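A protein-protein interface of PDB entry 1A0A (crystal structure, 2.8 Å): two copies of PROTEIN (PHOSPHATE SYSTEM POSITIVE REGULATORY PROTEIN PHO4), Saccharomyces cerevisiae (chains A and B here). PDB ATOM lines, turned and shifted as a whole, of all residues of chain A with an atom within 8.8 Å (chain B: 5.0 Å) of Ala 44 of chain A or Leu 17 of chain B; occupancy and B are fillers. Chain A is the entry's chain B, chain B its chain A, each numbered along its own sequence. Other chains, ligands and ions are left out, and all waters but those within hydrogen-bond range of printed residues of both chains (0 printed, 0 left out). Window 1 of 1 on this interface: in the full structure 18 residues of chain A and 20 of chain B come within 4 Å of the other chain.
Of the 9 printed residues of chain B, 5 touch a printed residue of chain A.
Hydrophobic or aromatic side chains of chain B within 4 Å of the printed part of chain A: Leu 17 and Ala 20.
Arg 14 of chain A touches its own counterpart, Arg 14 of chain B.
Positions printed for both chains: 14, 17 and 21.
Of the 10 pairs that touch across the chains among the printed residues, 1 has its exchanged pair printed and touching as well.
O of Ala 20 of chain B is in hydrogen-bond range of SG of Cys 51 of chain A, 3.7 Å away.
Among the printed residues, pairs that only touch across the chains: Arg 14 of chain A with Arg 14 of chain B (3.6 Å), Lys 43 of chain A with Leu 17 of chain B (3.2 Å), Ala 44 of chain A with Arg 16 of chain B (3.8 Å), Ala 44 of chain A with Leu 17 of chain B (2.9 Å), Ala 44 of chain A with Ala 20 of chain B (3.4 Å), Val 47 of chain A with Leu 17 of chain B (3.6 Å), Val 47 of chain A with Ala 20 of chain B (3.1 Å), Val 47 of chain A with Leu 21 of chain B (3.8 Å) and Glu 48 of chain A with Arg 16 of chain B (3.3 Å).
The guanidinium group (NH1) of Arg 16 of chain B lies within hydrogen-bond range of the side-chain amide oxygen (OD1) of Asn 15 of chain B, at 3.1 Å.
The side-chain carboxylate of Glu 48 of chain A is in hydrogen-bond range of the backbone NH of Thr 45 of chain A.
The backbone carbonyl oxygen (O) of Glu 48 of chain A lies close to the guanidinium group (NH1) of Arg 52 of chain A, at 3.1 Å.
Printed residues of chain B within 4 Å of Arg 14 of chain A: Arg 14.
Of the printed residues of chain B, Lys 43 of chain A touches Leu 17 (3.2 Å).
Of chain B, only Arg 16, Leu 17 and Ala 20 come within 4 Å of Ala 44 of chain A.
Of the printed residues of chain B, Glu 48 of chain A touches Arg 16.
Of the printed residues of chain A, Arg 16 of chain B touches Ala 44 and Glu 48.
The nearest printed residue of chain B that does not touch Ala 44 of chain A is Arg 13 of chain B (5.0 Å).
The nearest residue of chain A that does not touch Leu 17 of chain B is Leu 21 of chain A (4.7 Å).
The nearest printed residue of chain A that does not touch Ala 20 of chain B is Glu 48 of chain A (4.2 Å).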
ATOM      1  N   ARG A  14      -8.520  -9.791 -36.461  1.00  0.00           N
ATOM      2  CA  ARG A  14      -9.045  -8.861 -35.460  1.00  0.00           C
ATOM      3  C   ARG A  14      -9.528  -7.542 -36.044  1.00  0.00           C
ATOM      4  O   ARG A  14     -10.384  -6.867 -35.444  1.00  0.00           O
ATOM      5  CB  ARG A  14      -8.071  -8.595 -34.312  1.00  0.00           C
ATOM      6  CG  ARG A  14      -8.838  -8.082 -33.088  1.00  0.00           C
ATOM      7  CD  ARG A  14      -8.944  -9.104 -31.952  1.00  0.00           C
ATOM      8  NE  ARG A  14      -7.772  -8.932 -31.119  1.00  0.00           N
ATOM      9  CZ  ARG A  14      -7.561  -7.853 -30.372  1.00  0.00           C
ATOM     10  NH1 ARG A  14      -8.482  -6.889 -30.301  1.00  0.00           N
ATOM     11  NH2 ARG A  14      -6.322  -7.584 -29.971  1.00  0.00           N
ATOM     12  N   LEU A  17     -13.296  -7.446 -37.326  1.00  0.00           N
ATOM     13  CA  LEU A  17     -14.135  -7.128 -36.182  1.00  0.00           C
ATOM     14  C   LEU A  17     -14.314  -5.606 -36.074  1.00  0.00           C
ATOM     15  O   LEU A  17     -15.246  -5.134 -35.449  1.00  0.00           O
ATOM     16  CB  LEU A  17     -13.504  -7.695 -34.894  1.00  0.00           C
ATOM     17  CG  LEU A  17     -14.322  -8.013 -33.630  1.00  0.00           C
ATOM     18  CD1 LEU A  17     -13.879  -7.176 -32.431  1.00  0.00           C
ATOM     19  CD2 LEU A  17     -15.811  -7.818 -33.903  1.00  0.00           C
ATOM     20  N   LEU A  21     -17.914  -3.623 -37.326  1.00  0.00           N
ATOM     21  CA  LEU A  21     -18.348  -2.951 -36.113  1.00  0.00           C
ATOM     22  C   LEU A  21     -18.309  -1.471 -36.261  1.00  0.00           C
ATOM     23  O   LEU A  21     -19.140  -0.757 -35.703  1.00  0.00           O
ATOM     24  CB  LEU A  21     -17.422  -3.273 -34.964  1.00  0.00           C
ATOM     25  CG  LEU A  21     -17.755  -2.490 -33.704  1.00  0.00           C
ATOM     26  CD1 LEU A  21     -18.886  -3.188 -32.943  1.00  0.00           C
ATOM     27  CD2 LEU A  21     -16.515  -2.369 -32.882  1.00  0.00           C
ATOM     28  N   SER A  38     -22.462   6.886 -23.035  1.00  0.00           N
ATOM     29  CA  SER A  38     -21.398   6.555 -23.980  1.00  0.00           C
ATOM     30  C   SER A  38     -19.995   6.974 -23.533  1.00  0.00           C
ATOM     31  O   SER A  38     -19.625   8.156 -23.639  1.00  0.00           O
ATOM     32  CB  SER A  38     -21.719   7.129 -25.369  1.00  0.00           C
ATOM     33  OG  SER A  38     -22.211   8.463 -25.314  1.00  0.00           O
ATOM     34  N   ALA A  39     -19.252   6.017 -22.975  1.00  0.00           N
ATOM     35  CA  ALA A  39     -17.892   6.267 -22.503  1.00  0.00           C
ATOM     36  C   ALA A  39     -16.851   5.923 -23.567  1.00  0.00           C
ATOM     37  O   ALA A  39     -15.657   5.903 -23.264  1.00  0.00           O
ATOM     38  CB  ALA A  39     -17.623   5.478 -21.213  1.00  0.00           C
ATOM     39  N   ALA A  40     -17.298   5.783 -24.823  1.00  0.00           N
ATOM     40  CA  ALA A  40     -16.407   5.440 -25.934  1.00  0.00           C
ATOM     41  C   ALA A  40     -17.003   5.124 -27.283  1.00  0.00           C
ATOM     42  O   ALA A  40     -17.646   4.092 -27.488  1.00  0.00           O
ATOM     43  CB  ALA A  40     -15.596   4.242 -25.573  1.00  0.00           C
ATOM     44  N   PRO A  41     -16.616   5.914 -28.275  1.00  0.00           N
ATOM     45  CA  PRO A  41     -17.163   5.598 -29.578  1.00  0.00           C
ATOM     46  C   PRO A  41     -16.083   4.673 -30.133  1.00  0.00           C
ATOM     47  O   PRO A  41     -14.985   5.124 -30.484  1.00  0.00           O
ATOM     48  CB  PRO A  41     -17.180   6.960 -30.270  1.00  0.00           C
ATOM     49  CG  PRO A  41     -15.952   7.617 -29.742  1.00  0.00           C
ATOM     50  CD  PRO A  41     -15.971   7.241 -28.265  1.00  0.00           C
ATOM     51  N   SER A  42     -16.296   3.370 -29.995  1.00  0.00           N
ATOM     52  CA  SER A  42     -15.322   2.427 -30.538  1.00  0.00           C
ATOM     53  C   SER A  42     -15.833   0.980 -30.522  1.00  0.00           C
ATOM     54  O   SER A  42     -15.887   0.329 -31.570  1.00  0.00           O
ATOM     55  CB  SER A  42     -14.022   2.534 -29.700  1.00  0.00           C
ATOM     56  OG  SER A  42     -14.282   2.789 -28.310  1.00  0.00           O
ATOM     57  N   LYS A  43     -16.137   0.446 -29.345  1.00  0.00           N
ATOM     58  CA  LYS A  43     -16.734  -0.864 -29.300  1.00  0.00           C
ATOM     59  C   LYS A  43     -18.061  -0.890 -28.504  1.00  0.00           C
ATOM     60  O   LYS A  43     -19.034  -0.246 -28.897  1.00  0.00           O
ATOM     61  CB  LYS A  43     -15.669  -1.869 -28.873  1.00  0.00           C
ATOM     62  CG  LYS A  43     -15.067  -2.543 -30.093  1.00  0.00           C
ATOM     63  CD  LYS A  43     -13.590  -2.310 -30.274  1.00  0.00           C
ATOM     64  CE  LYS A  43     -12.774  -3.316 -29.450  1.00  0.00           C
ATOM     65  NZ  LYS A  43     -11.558  -3.851 -30.155  1.00  0.00           N
ATOM     66  N   ALA A  44     -18.102  -1.732 -27.466  1.00  0.00           N
ATOM     67  CA  ALA A  44     -19.179  -1.864 -26.468  1.00  0.00           C
ATOM     68  C   ALA A  44     -20.453  -0.986 -26.463  1.00  0.00           C
ATOM     69  O   ALA A  44     -21.551  -1.445 -26.781  1.00  0.00           O
ATOM     70  CB  ALA A  44     -18.576  -1.937 -25.076  1.00  0.00           C
ATOM     71  N   THR A  45     -20.266   0.276 -26.056  1.00  0.00           N
ATOM     72  CA  THR A  45     -21.326   1.291 -25.952  1.00  0.00           C
ATOM     73  C   THR A  45     -22.070   1.389 -27.252  1.00  0.00           C
ATOM     74  O   THR A  45     -23.272   1.159 -27.304  1.00  0.00           O
ATOM     75  CB  THR A  45     -20.751   2.703 -25.635  1.00  0.00           C
ATOM     76  OG1 THR A  45     -19.465   2.846 -26.259  1.00  0.00           O
ATOM     77  CG2 THR A  45     -20.651   2.944 -24.120  1.00  0.00           C
ATOM     78  N   THR A  46     -21.327   1.763 -28.289  1.00  0.00           N
ATOM     79  CA  THR A  46     -21.839   1.884 -29.635  1.00  0.00           C
ATOM     80  C   THR A  46     -22.673   0.644 -29.912  1.00  0.00           C
ATOM     81  O   THR A  46     -23.802   0.740 -30.360  1.00  0.00           O
ATOM     82  CB  THR A  46     -20.655   2.010 -30.641  1.00  0.00           C
ATOM     83  OG1 THR A  46     -20.438   3.391 -30.949  1.00  0.00           O
ATOM     84  CG2 THR A  46     -20.908   1.232 -31.919  1.00  0.00           C
ATOM     85  N   VAL A  47     -22.163  -0.513 -29.515  1.00  0.00           N
ATOM     86  CA  VAL A  47     -22.876  -1.758 -29.743  1.00  0.00           C
ATOM     87  C   VAL A  47     -24.101  -1.891 -28.837  1.00  0.00           C
ATOM     88  O   VAL A  47     -25.100  -2.486 -29.232  1.00  0.00           O
ATOM     89  CB  VAL A  47     -21.924  -2.962 -29.622  1.00  0.00           C
ATOM     90  CG1 VAL A  47     -22.512  -4.189 -30.323  1.00  0.00           C
ATOM     91  CG2 VAL A  47     -20.580  -2.604 -30.241  1.00  0.00           C
ATOM     92  N   GLU A  48     -24.038  -1.306 -27.638  1.00  0.00           N
ATOM     93  CA  GLU A  48     -25.174  -1.337 -26.718  1.00  0.00           C
ATOM     94  C   GLU A  48     -26.309  -0.649 -27.449  1.00  0.00           C
ATOM     95  O   GLU A  48     -27.362  -1.245 -27.648  1.00  0.00           O
ATOM     96  CB  GLU A  48     -24.853  -0.626 -25.401  1.00  0.00           C
ATOM     97  CG  GLU A  48     -24.050  -1.476 -24.420  1.00  0.00           C
ATOM     98  CD  GLU A  48     -22.830  -0.742 -23.875  1.00  0.00           C
ATOM     99  OE1 GLU A  48     -22.920   0.490 -23.696  1.00  0.00           O
ATOM    100  OE2 GLU A  48     -21.772  -1.380 -23.645  1.00  0.00           O
ATOM    101  N   ALA A  49     -26.046   0.562 -27.939  1.00  0.00           N
ATOM    102  CA  ALA A  49     -27.046   1.334 -28.697  1.00  0.00           C
ATOM    103  C   ALA A  49     -27.261   0.726 -30.092  1.00  0.00           C
ATOM    104  O   ALA A  49     -28.323   0.891 -30.704  1.00  0.00           O
ATOM    105  CB  ALA A  49     -26.644   2.824 -28.799  1.00  0.00           C
ATOM    106  N   ALA A  50     -26.264  -0.028 -30.551  1.00  0.00           N
ATOM    107  CA  ALA A  50     -26.313  -0.677 -31.854  1.00  0.00           C
ATOM    108  C   ALA A  50     -27.423  -1.715 -31.842  1.00  0.00           C
ATOM    109  O   ALA A  50     -28.058  -1.984 -32.863  1.00  0.00           O
ATOM    110  CB  ALA A  50     -24.975  -1.335 -32.162  1.00  0.00           C
ATOM    111  N   CYS A  51     -27.613  -2.335 -30.684  1.00  0.00           N
ATOM    112  CA  CYS A  51     -28.662  -3.311 -30.542  1.00  0.00           C
ATOM    113  C   CYS A  51     -29.962  -2.555 -30.360  1.00  0.00           C
ATOM    114  O   CYS A  51     -31.024  -3.016 -30.770  1.00  0.00           O
ATOM    115  CB  CYS A  51     -28.387  -4.221 -29.356  1.00  0.00           C
ATOM    116  SG  CYS A  51     -27.310  -5.590 -29.792  1.00  0.00           S
ATOM    117  N   ARG A  52     -29.845  -1.344 -29.824  1.00  0.00           N
ATOM    118  CA  ARG A  52     -30.990  -0.484 -29.572  1.00  0.00           C
ATOM    119  C   ARG A  52     -31.817  -0.105 -30.794  1.00  0.00           C
ATOM    120  O   ARG A  52     -32.958  -0.531 -30.865  1.00  0.00           O
ATOM    121  CB  ARG A  52     -30.552   0.731 -28.775  1.00  0.00           C
ATOM    122  CG  ARG A  52     -29.795   0.310 -27.531  1.00  0.00           C
ATOM    123  CD  ARG A  52     -30.158   1.087 -26.289  1.00  0.00           C
ATOM    124  NE  ARG A  52     -29.317   2.251 -26.033  1.00  0.00           N
ATOM    125  CZ  ARG A  52     -28.041   2.203 -25.668  1.00  0.00           C
ATOM    126  NH1 ARG A  52     -27.423   1.038 -25.541  1.00  0.00           N
ATOM    127  NH2 ARG A  52     -27.419   3.317 -25.299  1.00  0.00           N
ATOM    128  N   ARG B  13     -13.852  -4.529 -18.485  1.00  0.00           N
ATOM    129  CA  ARG B  13     -14.460  -3.460 -19.250  1.00  0.00           C
ATOM    130  C   ARG B  13     -14.867  -4.043 -20.621  1.00  0.00           C
ATOM    131  O   ARG B  13     -15.945  -3.721 -21.155  1.00  0.00           O
ATOM    132  CB  ARG B  13     -13.426  -2.352 -19.430  1.00  0.00           C
ATOM    133  CG  ARG B  13     -13.824  -1.181 -20.338  1.00  0.00           C
ATOM    134  CD  ARG B  13     -12.585  -0.387 -20.791  1.00  0.00           C
ATOM    135  NE  ARG B  13     -12.259  -0.538 -22.216  1.00  0.00           N
ATOM    136  CZ  ARG B  13     -11.969  -1.693 -22.821  1.00  0.00           C
ATOM    137  NH1 ARG B  13     -11.962  -2.840 -22.150  1.00  0.00           N
ATOM    138  NH2 ARG B  13     -11.645  -1.699 -24.107  1.00  0.00           N
ATOM    139  N   ARG B  14     -14.042  -4.976 -21.114  1.00  0.00           N
ATOM    140  CA  ARG B  14     -14.199  -5.659 -22.417  1.00  0.00           C
ATOM    141  C   ARG B  14     -15.481  -6.486 -22.454  1.00  0.00           C
ATOM    142  O   ARG B  14     -16.185  -6.522 -23.466  1.00  0.00           O
ATOM    143  CB  ARG B  14     -12.964  -6.567 -22.659  1.00  0.00           C
ATOM    144  CG  ARG B  14     -12.684  -7.141 -24.064  1.00  0.00           C
ATOM    145  CD  ARG B  14     -11.271  -7.778 -24.098  1.00  0.00           C
ATOM    146  NE  ARG B  14     -10.738  -8.030 -25.447  1.00  0.00           N
ATOM    147  CZ  ARG B  14      -9.448  -7.918 -25.809  1.00  0.00           C
ATOM    148  NH1 ARG B  14      -8.505  -7.542 -24.943  1.00  0.00           N
ATOM    149  NH2 ARG B  14      -9.082  -8.202 -27.054  1.00  0.00           N
ATOM    150  N   ASN B  15     -15.820  -7.048 -21.299  1.00  0.00           N
ATOM    151  CA  ASN B  15     -16.996  -7.893 -21.121  1.00  0.00           C
ATOM    152  C   ASN B  15     -18.225  -7.298 -21.789  1.00  0.00           C
ATOM    153  O   ASN B  15     -18.963  -7.986 -22.478  1.00  0.00           O
ATOM    154  CB  ASN B  15     -17.242  -8.173 -19.617  1.00  0.00           C
ATOM    155  CG  ASN B  15     -17.606  -6.917 -18.810  1.00  0.00           C
ATOM    156  OD1 ASN B  15     -17.293  -5.787 -19.194  1.00  0.00           O
ATOM    157  ND2 ASN B  15     -18.275  -7.126 -17.678  1.00  0.00           N
ATOM    158  N   ARG B  16     -18.393  -5.996 -21.625  1.00  0.00           N
ATOM    159  CA  ARG B  16     -19.514  -5.320 -22.227  1.00  0.00           C
ATOM    160  C   ARG B  16     -19.419  -5.545 -23.719  1.00  0.00           C
ATOM    161  O   ARG B  16     -20.270  -6.231 -24.287  1.00  0.00           O
ATOM    162  CB  ARG B  16     -19.510  -3.817 -21.908  1.00  0.00           C
ATOM    163  CG  ARG B  16     -20.505  -3.399 -20.836  1.00  0.00           C
ATOM    164  CD  ARG B  16     -20.454  -1.897 -20.658  1.00  0.00           C
ATOM    165  NE  ARG B  16     -20.318  -1.461 -19.276  1.00  0.00           N
ATOM    166  CZ  ARG B  16     -19.555  -2.051 -18.348  1.00  0.00           C
ATOM    167  NH1 ARG B  16     -18.827  -3.145 -18.624  1.00  0.00           N
ATOM    168  NH2 ARG B  16     -19.464  -1.495 -17.139  1.00  0.00           N
ATOM    169  N   LEU B  17     -18.327  -5.097 -24.332  1.00  0.00           N
ATOM    170  CA  LEU B  17     -18.210  -5.255 -25.760  1.00  0.00           C
ATOM    171  C   LEU B  17     -18.505  -6.694 -26.188  1.00  0.00           C
ATOM    172  O   LEU B  17     -19.024  -6.943 -27.292  1.00  0.00           O
ATOM    173  CB  LEU B  17     -16.850  -4.775 -26.248  1.00  0.00           C
ATOM    174  CG  LEU B  17     -16.722  -4.699 -27.779  1.00  0.00           C
ATOM    175  CD1 LEU B  17     -16.039  -5.941 -28.309  1.00  0.00           C
ATOM    176  CD2 LEU B  17     -18.078  -4.434 -28.476  1.00  0.00           C
ATOM    177  N   ALA B  18     -18.238  -7.639 -25.290  1.00  0.00           N
ATOM    178  CA  ALA B  18     -18.508  -9.041 -25.583  1.00  0.00           C
ATOM    179  C   ALA B  18     -20.023  -9.247 -25.831  1.00  0.00           C
ATOM    180  O   ALA B  18     -20.430  -9.619 -26.952  1.00  0.00           O
ATOM    181  CB  ALA B  18     -18.038  -9.906 -24.432  1.00  0.00           C
ATOM    182  N   VAL B  19     -20.834  -8.949 -24.800  1.00  0.00           N
ATOM    183  CA  VAL B  19     -22.299  -9.090 -24.841  1.00  0.00           C
ATOM    184  C   VAL B  19     -22.931  -8.066 -25.785  1.00  0.00           C
ATOM    185  O   VAL B  19     -24.027  -8.277 -26.266  1.00  0.00           O
ATOM    186  CB  VAL B  19     -22.980  -9.009 -23.421  1.00  0.00           C
ATOM    187  CG1 VAL B  19     -21.930  -9.002 -22.326  1.00  0.00           C
ATOM    188  CG2 VAL B  19     -23.884  -7.767 -23.289  1.00  0.00           C
ATOM    189  N   ALA B  20     -22.259  -6.939 -25.997  1.00  0.00           N
ATOM    190  CA  ALA B  20     -22.754  -5.936 -26.929  1.00  0.00           C
ATOM    191  C   ALA B  20     -22.839  -6.712 -28.218  1.00  0.00           C
ATOM    192  O   ALA B  20     -23.814  -6.645 -28.943  1.00  0.00           O
ATOM    193  CB  ALA B  20     -21.755  -4.818 -27.069  1.00  0.00           C
ATOM    194  N   LEU B  21     -21.798  -7.482 -28.478  1.00  0.00           N
ATOM    195  CA  LEU B  21     -21.790  -8.342 -29.627  1.00  0.00           C
ATOM    196  C   LEU B  21     -22.935  -9.342 -29.386  1.00  0.00           C
ATOM    197  O   LEU B  21     -23.660  -9.692 -30.320  1.00  0.00           O
ATOM    198  CB  LEU B  21     -20.446  -9.063 -29.716  1.00  0.00           C
ATOM    199  CG  LEU B  21     -19.659  -8.832 -31.005  1.00  0.00           C
ATOM    200  CD1 LEU B  21     -20.386  -9.499 -32.147  1.00  0.00           C
ATOM    201  CD2 LEU B  21     -19.479  -7.329 -31.252  1.00  0.00           C
